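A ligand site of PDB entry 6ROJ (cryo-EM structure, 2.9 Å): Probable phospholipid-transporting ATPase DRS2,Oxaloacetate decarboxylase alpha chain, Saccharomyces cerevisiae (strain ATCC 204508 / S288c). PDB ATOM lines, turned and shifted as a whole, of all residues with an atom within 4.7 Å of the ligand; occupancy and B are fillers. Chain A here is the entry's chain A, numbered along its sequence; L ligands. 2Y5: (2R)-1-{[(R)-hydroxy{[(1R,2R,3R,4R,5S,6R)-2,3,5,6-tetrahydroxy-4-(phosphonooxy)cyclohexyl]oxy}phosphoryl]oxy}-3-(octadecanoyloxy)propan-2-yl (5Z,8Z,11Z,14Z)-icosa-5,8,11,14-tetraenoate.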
ATOM      1  N   VAL A 454      -3.111 -12.491 -21.271  1.00  0.00           N
ATOM      2  CA  VAL A 454      -3.656 -12.942 -19.992  1.00  0.00           C
ATOM      3  C   VAL A 454      -2.619 -12.739 -18.898  1.00  0.00           C
ATOM      4  O   VAL A 454      -2.940 -12.286 -17.794  1.00  0.00           O
ATOM      5  CB  VAL A 454      -4.123 -14.395 -20.088  1.00  0.00           C
ATOM      6  CG1 VAL A 454      -4.460 -14.970 -18.728  1.00  0.00           C
ATOM      7  CG2 VAL A 454      -5.340 -14.482 -20.947  1.00  0.00           C
ATOM      8  N   VAL A 457      -2.226  -9.115 -17.639  1.00  0.00           N
ATOM      9  CA  VAL A 457      -3.344  -8.707 -16.799  1.00  0.00           C
ATOM     10  C   VAL A 457      -3.154  -9.141 -15.347  1.00  0.00           C
ATOM     11  O   VAL A 457      -3.307  -8.335 -14.429  1.00  0.00           O
ATOM     12  CB  VAL A 457      -4.661  -9.247 -17.386  1.00  0.00           C
ATOM     13  CG1 VAL A 457      -5.777  -9.233 -16.363  1.00  0.00           C
ATOM     14  CG2 VAL A 457      -5.055  -8.424 -18.597  1.00  0.00           C
ATOM     15  N   LEU A 458      -2.774 -10.401 -15.128  1.00  0.00           N
ATOM     16  CA  LEU A 458      -2.623 -10.907 -13.756  1.00  0.00           C
ATOM     17  C   LEU A 458      -1.396 -10.320 -13.065  1.00  0.00           C
ATOM     18  O   LEU A 458      -1.380 -10.181 -11.839  1.00  0.00           O
ATOM     19  CB  LEU A 458      -2.552 -12.429 -13.776  1.00  0.00           C
ATOM     20  CG  LEU A 458      -3.616 -13.021 -14.688  1.00  0.00           C
ATOM     21  CD1 LEU A 458      -3.226 -14.407 -15.096  1.00  0.00           C
ATOM     22  CD2 LEU A 458      -4.969 -13.022 -14.036  1.00  0.00           C
ATOM     23  N   TRP A1028      -4.883 -17.045  -7.299  1.00  0.00           N
ATOM     24  CA  TRP A1028      -5.932 -16.848  -6.317  1.00  0.00           C
ATOM     25  C   TRP A1028      -5.397 -16.723  -4.901  1.00  0.00           C
ATOM     26  O   TRP A1028      -6.132 -16.311  -4.001  1.00  0.00           O
ATOM     27  CB  TRP A1028      -6.964 -17.966  -6.379  1.00  0.00           C
ATOM     28  CG  TRP A1028      -7.457 -18.350  -7.764  1.00  0.00           C
ATOM     29  CD1 TRP A1028      -7.506 -19.602  -8.275  1.00  0.00           C
ATOM     30  CD2 TRP A1028      -8.010 -17.487  -8.777  1.00  0.00           C
ATOM     31  NE1 TRP A1028      -8.025 -19.583  -9.544  1.00  0.00           N
ATOM     32  CE2 TRP A1028      -8.337 -18.296  -9.871  1.00  0.00           C
ATOM     33  CE3 TRP A1028      -8.243 -16.105  -8.867  1.00  0.00           C
ATOM     34  CZ2 TRP A1028      -8.892 -17.779 -11.037  1.00  0.00           C
ATOM     35  CZ3 TRP A1028      -8.779 -15.597 -10.026  1.00  0.00           C
ATOM     36  CH2 TRP A1028      -9.102 -16.433 -11.094  1.00  0.00           C
ATOM     37  N   PHE A1031      -4.659 -12.836  -3.148  1.00  0.00           N
ATOM     38  CA  PHE A1031      -5.666 -12.138  -2.367  1.00  0.00           C
ATOM     39  C   PHE A1031      -5.703 -12.603  -0.912  1.00  0.00           C
ATOM     40  O   PHE A1031      -6.413 -12.008  -0.107  1.00  0.00           O
ATOM     41  CB  PHE A1031      -7.037 -12.320  -3.011  1.00  0.00           C
ATOM     42  CG  PHE A1031      -7.080 -11.880  -4.436  1.00  0.00           C
ATOM     43  CD1 PHE A1031      -7.075 -10.527  -4.753  1.00  0.00           C
ATOM     44  CD2 PHE A1031      -7.133 -12.806  -5.461  1.00  0.00           C
ATOM     45  CE1 PHE A1031      -7.112 -10.122  -6.067  1.00  0.00           C
ATOM     46  CE2 PHE A1031      -7.170 -12.401  -6.775  1.00  0.00           C
ATOM     47  CZ  PHE A1031      -7.155 -11.048  -7.077  1.00  0.00           C
ATOM     48  N   TYR A1092     -10.092 -20.042 -30.699  1.00  0.00           N
ATOM     49  CA  TYR A1092     -11.390 -20.068 -30.016  1.00  0.00           C
ATOM     50  C   TYR A1092     -11.568 -21.351 -29.203  1.00  0.00           C
ATOM     51  O   TYR A1092     -12.168 -21.325 -28.132  1.00  0.00           O
ATOM     52  CB  TYR A1092     -12.513 -19.913 -31.029  1.00  0.00           C
ATOM     53  CG  TYR A1092     -13.895 -19.958 -30.435  1.00  0.00           C
ATOM     54  CD1 TYR A1092     -14.419 -18.853 -29.786  1.00  0.00           C
ATOM     55  CD2 TYR A1092     -14.682 -21.099 -30.542  1.00  0.00           C
ATOM     56  CE1 TYR A1092     -15.694 -18.885 -29.243  1.00  0.00           C
ATOM     57  CE2 TYR A1092     -15.951 -21.139 -29.996  1.00  0.00           C
ATOM     58  CZ  TYR A1092     -16.452 -20.029 -29.350  1.00  0.00           C
ATOM     59  OH  TYR A1092     -17.717 -20.071 -28.814  1.00  0.00           O
ATOM     60  N   ILE A1093     -11.057 -22.479 -29.706  1.00  0.00           N
ATOM     61  CA  ILE A1093     -11.057 -23.697 -28.917  1.00  0.00           C
ATOM     62  C   ILE A1093     -10.012 -23.601 -27.808  1.00  0.00           C
ATOM     63  O   ILE A1093     -10.186 -24.180 -26.733  1.00  0.00           O
ATOM     64  CB  ILE A1093     -10.823 -24.925 -29.825  1.00  0.00           C
ATOM     65  CG1 ILE A1093     -11.858 -24.952 -30.949  1.00  0.00           C
ATOM     66  CG2 ILE A1093     -10.952 -26.232 -29.078  1.00  0.00           C
ATOM     67  CD1 ILE A1093     -11.285 -24.667 -32.306  1.00  0.00           C
ATOM     68  N   TRP A1095      -9.302 -20.964 -26.021  1.00  0.00           N
ATOM     69  CA  TRP A1095      -9.835 -20.228 -24.880  1.00  0.00           C
ATOM     70  C   TRP A1095     -10.680 -21.101 -23.978  1.00  0.00           C
ATOM     71  O   TRP A1095     -10.805 -20.806 -22.783  1.00  0.00           O
ATOM     72  CB  TRP A1095     -10.678 -19.049 -25.345  1.00  0.00           C
ATOM     73  CG  TRP A1095      -9.888 -17.854 -25.750  1.00  0.00           C
ATOM     74  CD1 TRP A1095      -9.842 -17.288 -26.981  1.00  0.00           C
ATOM     75  CD2 TRP A1095      -9.029 -17.067 -24.916  1.00  0.00           C
ATOM     76  NE1 TRP A1095      -9.009 -16.203 -26.980  1.00  0.00           N
ATOM     77  CE2 TRP A1095      -8.494 -16.045 -25.722  1.00  0.00           C
ATOM     78  CE3 TRP A1095      -8.656 -17.122 -23.574  1.00  0.00           C
ATOM     79  CZ2 TRP A1095      -7.619 -15.092 -25.228  1.00  0.00           C
ATOM     80  CZ3 TRP A1095      -7.789 -16.175 -23.082  1.00  0.00           C
ATOM     81  CH2 TRP A1095      -7.278 -15.181 -23.914  1.00  0.00           C
ATOM     82  N   GLY A1096     -11.264 -22.182 -24.502  1.00  0.00           N
ATOM     83  CA  GLY A1096     -12.072 -23.036 -23.664  1.00  0.00           C
ATOM     84  C   GLY A1096     -11.268 -24.003 -22.823  1.00  0.00           C
ATOM     85  O   GLY A1096     -11.783 -24.574 -21.870  1.00  0.00           O
ATOM     86  N   ILE A1099     -10.201 -21.359 -19.928  1.00  0.00           N
ATOM     87  CA  ILE A1099     -11.338 -21.061 -19.060  1.00  0.00           C
ATOM     88  C   ILE A1099     -11.764 -22.297 -18.279  1.00  0.00           C
ATOM     89  O   ILE A1099     -12.215 -22.183 -17.138  1.00  0.00           O
ATOM     90  CB  ILE A1099     -12.456 -20.438 -19.923  1.00  0.00           C
ATOM     91  CG1 ILE A1099     -12.065 -19.028 -20.332  1.00  0.00           C
ATOM     92  CG2 ILE A1099     -13.778 -20.353 -19.207  1.00  0.00           C
ATOM     93  CD1 ILE A1099     -12.980 -18.402 -21.331  1.00  0.00           C
ATOM     94  N   ASN A1100     -11.536 -23.490 -18.824  1.00  0.00           N
ATOM     95  CA  ASN A1100     -11.687 -24.681 -18.002  1.00  0.00           C
ATOM     96  C   ASN A1100     -10.540 -24.827 -17.014  1.00  0.00           C
ATOM     97  O   ASN A1100     -10.710 -25.451 -15.964  1.00  0.00           O
ATOM     98  CB  ASN A1100     -11.780 -25.928 -18.877  1.00  0.00           C
ATOM     99  CG  ASN A1100     -12.523 -27.044 -18.212  1.00  0.00           C
ATOM    100  OD1 ASN A1100     -13.144 -26.848 -17.166  1.00  0.00           O
ATOM    101  ND2 ASN A1100     -12.469 -28.228 -18.792  1.00  0.00           N
ATOM    102  N   PHE A1102      -8.992 -22.132 -15.597  1.00  0.00           N
ATOM    103  CA  PHE A1102      -9.334 -21.168 -14.567  1.00  0.00           C
ATOM    104  C   PHE A1102     -10.430 -21.707 -13.656  1.00  0.00           C
ATOM    105  O   PHE A1102     -10.415 -21.483 -12.451  1.00  0.00           O
ATOM    106  CB  PHE A1102      -9.795 -19.850 -15.178  1.00  0.00           C
ATOM    107  CG  PHE A1102      -8.706 -19.034 -15.815  1.00  0.00           C
ATOM    108  CD1 PHE A1102      -7.373 -19.371 -15.685  1.00  0.00           C
ATOM    109  CD2 PHE A1102      -9.035 -17.912 -16.562  1.00  0.00           C
ATOM    110  CE1 PHE A1102      -6.390 -18.612 -16.287  1.00  0.00           C
ATOM    111  CE2 PHE A1102      -8.052 -17.152 -17.164  1.00  0.00           C
ATOM    112  CZ  PHE A1102      -6.732 -17.494 -17.017  1.00  0.00           C
ATOM    113  N   PHE A1103     -11.401 -22.399 -14.242  1.00  0.00           N
ATOM    114  CA  PHE A1103     -12.513 -22.931 -13.464  1.00  0.00           C
ATOM    115  C   PHE A1103     -12.074 -24.077 -12.583  1.00  0.00           C
ATOM    116  O   PHE A1103     -12.550 -24.211 -11.454  1.00  0.00           O
ATOM    117  CB  PHE A1103     -13.638 -23.383 -14.401  1.00  0.00           C
ATOM    118  CG  PHE A1103     -14.781 -24.032 -13.694  1.00  0.00           C
ATOM    119  CD1 PHE A1103     -15.645 -23.285 -12.904  1.00  0.00           C
ATOM    120  CD2 PHE A1103     -15.026 -25.386 -13.846  1.00  0.00           C
ATOM    121  CE1 PHE A1103     -16.696 -23.884 -12.257  1.00  0.00           C
ATOM    122  CE2 PHE A1103     -16.085 -25.991 -13.201  1.00  0.00           C
ATOM    123  CZ  PHE A1103     -16.917 -25.233 -12.412  1.00  0.00           C
ATOM    124  N   ALA A1106     -10.058 -22.719  -9.568  1.00  0.00           N
ATOM    125  CA  ALA A1106     -10.846 -22.028  -8.546  1.00  0.00           C
ATOM    126  C   ALA A1106     -11.594 -23.008  -7.676  1.00  0.00           C
ATOM    127  O   ALA A1106     -11.913 -22.708  -6.523  1.00  0.00           O
ATOM    128  CB  ALA A1106     -11.807 -21.051  -9.207  1.00  0.00           C
ATOM    129  N   ILE A1110     -10.727 -22.464  -3.705  1.00  0.00           N
ATOM    130  CA  ILE A1110     -11.841 -22.134  -2.833  1.00  0.00           C
ATOM    131  C   ILE A1110     -12.361 -23.370  -2.104  1.00  0.00           C
ATOM    132  O   ILE A1110     -12.853 -23.282  -0.983  1.00  0.00           O
ATOM    133  CB  ILE A1110     -12.945 -21.430  -3.648  1.00  0.00           C
ATOM    134  CG1 ILE A1110     -12.352 -20.207  -4.352  1.00  0.00           C
ATOM    135  CG2 ILE A1110     -14.073 -20.927  -2.778  1.00  0.00           C
ATOM    136  CD1 ILE A1110     -13.298 -19.531  -5.292  1.00  0.00           C
ATOM    137  N   LEU A1152     -11.021 -38.404 -19.749  1.00  0.00           N
ATOM    138  CA  LEU A1152     -12.229 -38.121 -20.518  1.00  0.00           C
ATOM    139  C   LEU A1152     -11.894 -37.758 -21.950  1.00  0.00           C
ATOM    140  O   LEU A1152     -12.721 -37.977 -22.848  1.00  0.00           O
ATOM    141  CB  LEU A1152     -13.006 -36.967 -19.882  1.00  0.00           C
ATOM    142  CG  LEU A1152     -13.683 -37.249 -18.548  1.00  0.00           C
ATOM    143  CD1 LEU A1152     -13.943 -35.955 -17.834  1.00  0.00           C
ATOM    144  CD2 LEU A1152     -14.976 -38.007 -18.765  1.00  0.00           C
ATOM    145  N   ASN A1155      -9.903 -41.497 -26.368  1.00  0.00           N
ATOM    146  CA  ASN A1155     -10.924 -42.252 -27.090  1.00  0.00           C
ATOM    147  C   ASN A1155     -10.738 -43.760 -26.959  1.00  0.00           C
ATOM    148  O   ASN A1155     -11.723 -44.500 -26.952  1.00  0.00           O
ATOM    149  CB  ASN A1155     -10.915 -41.856 -28.568  1.00  0.00           C
ATOM    150  CG  ASN A1155     -10.960 -40.368 -28.768  1.00  0.00           C
ATOM    151  OD1 ASN A1155     -12.031 -39.768 -28.810  1.00  0.00           O
ATOM    152  ND2 ASN A1155      -9.797 -39.752 -28.915  1.00  0.00           N
ATOM    153  N   ARG A1219     -18.704 -31.080 -14.731  1.00  0.00           N
ATOM    154  CA  ARG A1219     -19.132 -30.298 -15.875  1.00  0.00           C
ATOM    155  C   ARG A1219     -18.541 -30.845 -17.166  1.00  0.00           C
ATOM    156  O   ARG A1219     -19.181 -30.774 -18.215  1.00  0.00           O
ATOM    157  CB  ARG A1219     -18.750 -28.835 -15.681  1.00  0.00           C
ATOM    158  CG  ARG A1219     -19.683 -27.825 -16.347  1.00  0.00           C
ATOM    159  CD  ARG A1219     -19.232 -27.510 -17.757  1.00  0.00           C
ATOM    160  NE  ARG A1219     -17.795 -27.315 -17.801  1.00  0.00           N
ATOM    161  CZ  ARG A1219     -17.044 -27.613 -18.857  1.00  0.00           C
ATOM    162  NH1 ARG A1219     -15.732 -27.405 -18.816  1.00  0.00           N
ATOM    163  NH2 ARG A1219     -17.596 -28.132 -19.940  1.00  0.00           N
ATOM    164  N   ASP A1220     -17.321 -31.375 -17.105  1.00  0.00           N
ATOM    165  CA  ASP A1220     -16.710 -31.973 -18.290  1.00  0.00           C
ATOM    166  C   ASP A1220     -17.339 -33.313 -18.630  1.00  0.00           C
ATOM    167  O   ASP A1220     -17.304 -33.752 -19.775  1.00  0.00           O
ATOM    168  CB  ASP A1220     -15.206 -32.124 -18.084  1.00  0.00           C
ATOM    169  CG  ASP A1220     -14.481 -30.806 -18.080  1.00  0.00           C
ATOM    170  OD1 ASP A1220     -14.945 -29.885 -18.764  1.00  0.00           O
ATOM    171  OD2 ASP A1220     -13.459 -30.696 -17.392  1.00  0.00           O
ATOM    172  N   TRP A1223     -21.172 -32.572 -20.022  1.00  0.00           N
ATOM    173  CA  TRP A1223     -21.208 -32.005 -21.364  1.00  0.00           C
ATOM    174  C   TRP A1223     -20.765 -33.022 -22.398  1.00  0.00           C
ATOM    175  O   TRP A1223     -21.194 -32.968 -23.546  1.00  0.00           O
ATOM    176  CB  TRP A1223     -20.344 -30.750 -21.436  1.00  0.00           C
ATOM    177  CG  TRP A1223     -20.343 -30.145 -22.791  1.00  0.00           C
ATOM    178  CD1 TRP A1223     -19.336 -30.189 -23.697  1.00  0.00           C
ATOM    179  CD2 TRP A1223     -21.407 -29.417 -23.405  1.00  0.00           C
ATOM    180  NE1 TRP A1223     -19.692 -29.521 -24.837  1.00  0.00           N
ATOM    181  CE2 TRP A1223     -20.963 -29.034 -24.688  1.00  0.00           C
ATOM    182  CE3 TRP A1223     -22.684 -29.053 -23.001  1.00  0.00           C
ATOM    183  CZ2 TRP A1223     -21.757 -28.304 -25.553  1.00  0.00           C
ATOM    184  CZ3 TRP A1223     -23.478 -28.323 -23.866  1.00  0.00           C
ATOM    185  CH2 TRP A1223     -23.006 -27.963 -25.127  1.00  0.00           C
ATOM    186  N   LYS A1224     -19.918 -33.971 -21.999  1.00  0.00           N
ATOM    187  CA  LYS A1224     -19.507 -35.027 -22.923  1.00  0.00           C
ATOM    188  C   LYS A1224     -20.668 -35.963 -23.226  1.00  0.00           C
ATOM    189  O   LYS A1224     -20.740 -36.536 -24.327  1.00  0.00           O
ATOM    190  CB  LYS A1224     -18.328 -35.805 -22.330  1.00  0.00           C
ATOM    191  CG  LYS A1224     -17.599 -36.701 -23.316  1.00  0.00           C
ATOM    192  CD  LYS A1224     -16.624 -37.613 -22.616  1.00  0.00           C
ATOM    193  CE  LYS A1224     -15.865 -38.449 -23.610  1.00  0.00           C
ATOM    194  NZ  LYS A1224     -14.870 -37.646 -24.371  1.00  0.00           N
ATOM    195  N   LYS A1227     -23.144 -33.655 -25.505  1.00  0.00           N
ATOM    196  CA  LYS A1227     -22.658 -33.367 -26.849  1.00  0.00           C
ATOM    197  C   LYS A1227     -22.844 -34.536 -27.783  1.00  0.00           C
ATOM    198  O   LYS A1227     -23.230 -34.358 -28.941  1.00  0.00           O
ATOM    199  CB  LYS A1227     -21.186 -32.956 -26.810  1.00  0.00           C
ATOM    200  CG  LYS A1227     -20.646 -32.458 -28.127  1.00  0.00           C
ATOM    201  CD  LYS A1227     -21.057 -31.032 -28.365  1.00  0.00           C
ATOM    202  CE  LYS A1227     -20.585 -30.536 -29.725  1.00  0.00           C
ATOM    203  NZ  LYS A1227     -21.516 -30.928 -30.806  1.00  0.00           N
ATOM    204  N   TYR A1235     -18.366 -36.809 -36.790  1.00  0.00           N
ATOM    205  CA  TYR A1235     -17.507 -37.924 -36.401  1.00  0.00           C
ATOM    206  C   TYR A1235     -17.987 -38.618 -35.137  1.00  0.00           C
ATOM    207  O   TYR A1235     -17.510 -39.713 -34.852  1.00  0.00           O
ATOM    208  CB  TYR A1235     -16.055 -37.450 -36.217  1.00  0.00           C
ATOM    209  CG  TYR A1235     -15.818 -36.486 -35.084  1.00  0.00           C
ATOM    210  CD1 TYR A1235     -15.987 -35.125 -35.258  1.00  0.00           C
ATOM    211  CD2 TYR A1235     -15.361 -36.937 -33.852  1.00  0.00           C
ATOM    212  CE1 TYR A1235     -15.767 -34.238 -34.228  1.00  0.00           C
ATOM    213  CE2 TYR A1235     -15.135 -36.057 -32.820  1.00  0.00           C
ATOM    214  CZ  TYR A1235     -15.330 -34.709 -33.010  1.00  0.00           C
ATOM    215  OH  TYR A1235     -15.095 -33.838 -31.984  1.00  0.00           O
ATOM    216  N   HIS A1236     -18.918 -38.017 -34.384  1.00  0.00           N
ATOM    217  CA  HIS A1236     -19.456 -38.683 -33.206  1.00  0.00           C
ATOM    218  C   HIS A1236     -20.362 -39.845 -33.591  1.00  0.00           C
ATOM    219  O   HIS A1236     -20.570 -40.762 -32.797  1.00  0.00           O
ATOM    220  CB  HIS A1236     -20.219 -37.684 -32.336  1.00  0.00           C
ATOM    221  CG  HIS A1236     -19.344 -36.740 -31.577  1.00  0.00           C
ATOM    222  ND1 HIS A1236     -19.190 -35.428 -31.926  1.00  0.00           N
ATOM    223  CD2 HIS A1236     -18.586 -36.933 -30.466  1.00  0.00           C
ATOM    224  CE1 HIS A1236     -18.369 -34.834 -31.071  1.00  0.00           C
ATOM    225  NE2 HIS A1236     -17.986 -35.730 -30.183  1.00  0.00           N
ATOM    226  N   GLN A1239     -17.919 -42.725 -34.715  1.00  0.00           N
ATOM    227  CA  GLN A1239     -17.385 -43.379 -33.519  1.00  0.00           C
ATOM    228  C   GLN A1239     -18.415 -44.319 -32.913  1.00  0.00           C
ATOM    229  O   GLN A1239     -18.053 -45.334 -32.304  1.00  0.00           O
ATOM    230  CB  GLN A1239     -16.938 -42.347 -32.506  1.00  0.00           C
ATOM    231  CG  GLN A1239     -15.699 -41.580 -32.910  1.00  0.00           C
ATOM    232  CD  GLN A1239     -15.219 -40.633 -31.835  1.00  0.00           C
ATOM    233  OE1 GLN A1239     -15.624 -40.730 -30.687  1.00  0.00           O
ATOM    234  NE2 GLN A1239     -14.354 -39.701 -32.218  1.00  0.00           N
HETATM  235  C1  2Y5 L   1     -15.939 -30.722 -25.712  1.00  0.00           C
HETATM  236  O1  2Y5 L   1     -15.041 -30.079 -24.849  1.00  0.00           O
HETATM  237  P1  2Y5 L   1     -15.646 -29.057 -23.709  1.00  0.00           P
HETATM  238  C2  2Y5 L   1     -16.423 -32.040 -25.068  1.00  0.00           C
HETATM  239  O2  2Y5 L   1     -15.745 -32.246 -23.854  1.00  0.00           O
HETATM  240  C3  2Y5 L   1     -16.251 -33.326 -25.895  1.00  0.00           C
HETATM  241  O3  2Y5 L   1     -17.249 -34.220 -25.485  1.00  0.00           O
HETATM  242  C4  2Y5 L   1     -16.337 -33.196 -27.427  1.00  0.00           C
HETATM  243  O4  2Y5 L   1     -15.347 -34.025 -27.988  1.00  0.00           O
HETATM  244  P4  2Y5 L   1     -15.396 -35.667 -27.791  1.00  0.00           P
HETATM  245  C5  2Y5 L   1     -16.126 -31.785 -27.990  1.00  0.00           C
HETATM  246  O5  2Y5 L   1     -17.377 -31.159 -28.156  1.00  0.00           O
HETATM  247  C6  2Y5 L   1     -15.274 -30.898 -27.084  1.00  0.00           C
HETATM  248  O6  2Y5 L   1     -15.141 -29.632 -27.698  1.00  0.00           O
HETATM  249  C7  2Y5 L   1     -14.241 -26.977 -24.341  1.00  0.00           C
HETATM  250  C8  2Y5 L   1     -15.039 -25.694 -24.106  1.00  0.00           C
HETATM  251  C9  2Y5 L   1     -14.885 -25.260 -22.657  1.00  0.00           C
HETATM  252  C10 2Y5 L   1     -15.224 -24.477 -26.139  1.00  0.00           C
HETATM  253  C11 2Y5 L   1     -16.194 -24.032 -21.144  1.00  0.00           C
HETATM  254  O11 2Y5 L   1     -15.981 -29.863 -22.482  1.00  0.00           O
HETATM  255  C12 2Y5 L   1     -16.176 -23.292 -26.207  1.00  0.00           C
HETATM  256  O12 2Y5 L   1     -16.895 -28.402 -24.237  1.00  0.00           O
HETATM  257  C13 2Y5 L   1     -15.379 -22.026 -26.502  1.00  0.00           C
HETATM  258  O13 2Y5 L   1     -14.531 -27.912 -23.349  1.00  0.00           O
HETATM  259  C14 2Y5 L   1     -15.175 -21.238 -25.202  1.00  0.00           C
HETATM  260  C15 2Y5 L   1     -16.390 -20.363 -24.940  1.00  0.00           C
HETATM  261  C16 2Y5 L   1     -16.288 -19.088 -24.626  1.00  0.00           C
HETATM  262  O16 2Y5 L   1     -14.523 -24.716 -24.957  1.00  0.00           O
HETATM  263  C17 2Y5 L   1     -14.930 -18.395 -24.507  1.00  0.00           C
HETATM  264  O17 2Y5 L   1     -15.055 -25.172 -27.075  1.00  0.00           O
HETATM  265  C18 2Y5 L   1     -14.592 -17.667 -25.810  1.00  0.00           C
HETATM  266  O18 2Y5 L   1     -16.119 -25.133 -22.013  1.00  0.00           O
HETATM  267  C19 2Y5 L   1     -13.723 -16.674 -25.850  1.00  0.00           C
HETATM  268  O19 2Y5 L   1     -16.592 -22.998 -21.545  1.00  0.00           O
HETATM  269  C20 2Y5 L   1     -13.022 -16.173 -24.591  1.00  0.00           C
HETATM  270  C21 2Y5 L   1     -12.560 -14.736 -24.822  1.00  0.00           C
HETATM  271  C22 2Y5 L   1     -11.833 -14.087 -23.941  1.00  0.00           C
HETATM  272  C23 2Y5 L   1     -11.400 -14.735 -22.620  1.00  0.00           C
HETATM  273  C24 2Y5 L   1     -12.160 -14.080 -21.469  1.00  0.00           C
HETATM  274  C25 2Y5 L   1     -11.574 -13.719 -20.348  1.00  0.00           C
HETATM  275  C26 2Y5 L   1     -10.080 -13.930 -20.107  1.00  0.00           C
HETATM  276  C27 2Y5 L   1      -9.599 -12.868 -19.118  1.00  0.00           C
HETATM  277  C28 2Y5 L   1      -8.334 -13.341 -18.415  1.00  0.00           C
HETATM  278  C29 2Y5 L   1      -7.798 -12.221 -17.531  1.00  0.00           C
HETATM  279  C30 2Y5 L   1      -8.132 -12.517 -16.063  1.00  0.00           C
HETATM  280  C31 2Y5 L   1     -15.774 -24.162 -19.674  1.00  0.00           C
HETATM  281  C32 2Y5 L   1     -16.994 -23.946 -18.781  1.00  0.00           C
HETATM  282  C33 2Y5 L   1     -16.559 -23.546 -17.375  1.00  0.00           C
HETATM  283  C34 2Y5 L   1     -16.504 -22.019 -17.283  1.00  0.00           C
HETATM  284  C35 2Y5 L   1     -16.873 -21.544 -15.869  1.00  0.00           C
HETATM  285  C36 2Y5 L   1     -16.457 -20.086 -15.685  1.00  0.00           C
HETATM  286  C37 2Y5 L   1     -15.048 -20.006 -15.112  1.00  0.00           C
HETATM  287  C38 2Y5 L   1     -14.722 -18.570 -14.690  1.00  0.00           C
HETATM  288  C39 2Y5 L   1     -13.440 -18.535 -13.858  1.00  0.00           C
HETATM  289  C40 2Y5 L   1     -13.769 -18.731 -12.378  1.00  0.00           C
HETATM  290  C41 2Y5 L   1     -12.974 -17.749 -11.523  1.00  0.00           C
HETATM  291  O41 2Y5 L   1     -14.547 -36.079 -26.605  1.00  0.00           O
HETATM  292  C42 2Y5 L   1     -13.697 -17.541 -10.194  1.00  0.00           C
HETATM  293  O42 2Y5 L   1     -16.816 -36.123 -27.596  1.00  0.00           O
HETATM  294  C43 2Y5 L   1     -13.004 -16.470  -9.349  1.00  0.00           C
HETATM  295  O43 2Y5 L   1     -14.833 -36.321 -29.027  1.00  0.00           O
HETATM  296  C44 2Y5 L   1     -12.444 -17.086  -8.065  1.00  0.00           C
HETATM  297  C45 2Y5 L   1     -11.574 -16.065  -7.337  1.00  0.00           C
HETATM  298  C46 2Y5 L   1     -10.976 -16.700  -6.081  1.00  0.00           C
HETATM  299  C47 2Y5 L   1     -10.635 -15.627  -5.054  1.00  0.00           C
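The side-chain carboxylate of Asp 1220 sits at hydrogen-bond distance from the side-chain amide nitrogen of Asn 1100, at 3.0 Å.
The guanidinium group (NH1) of Arg 1219 lies within salt-bridge range of the side-chain carboxylate (OD1) of Asp 1220 (2.6 Å).
NZ of Lys 1224 lies within hydrogen-bond range of O of Leu 1152.
The guanidinium group of Arg 1219 sits at hydrogen-bond distance from the side-chain amide oxygen of Asn 1100 (3.1 Å).
Merely in contact with the ligand: Val 457 (3.8 Å), Leu 458 (3.8 Å), Trp 1028 (3.7 Å), Tyr 1092 (3.6 Å), Trp 1095 (3.7 Å), Gly 1096 (3.2 Å), Ile 1099 (3.7 Å), Phe 1103 (3.7 Å), Ile 1110 (3.7 Å), Asp 1220 (3.9 Å), Lys 1227 (3.5 Å) and Tyr 1235 (3.8 Å).
Hydrophobic or aromatic side chains within 4 Å of the ligand: Val 457, Leu 458, Trp 1028, Tyr 1092, Trp 1095, Ile 1099, Phe 1103, Ile 1110, Trp 1223, Tyr 1235 and His 1236.
16 residues have an atom within 4 Å of the ligand: Val 457, Leu 458, Trp 1028, Tyr 1092, Trp 1095, Gly 1096, Ile 1099, Phe 1103, Ile 1110, Arg 1219, Asp 1220, Trp 1223, Lys 1224, Lys 1227, Tyr 1235 and His 1236.
O42 of the ligand lies within hydrogen-bond range of NE2 of His 1236 (2.9 Å).
The side-chain amino group (NZ) of Lys 1224 lies within salt-bridge range of an oxygen (O41) of the ligand, at 2.7 Å.
NE1 of Trp 1223 sits at hydrogen-bond distance from O12 of the ligand, at 3.1 Å.
NH2 of Arg 1219 lies within salt-bridge range of O11 of the ligand (3.5 Å).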
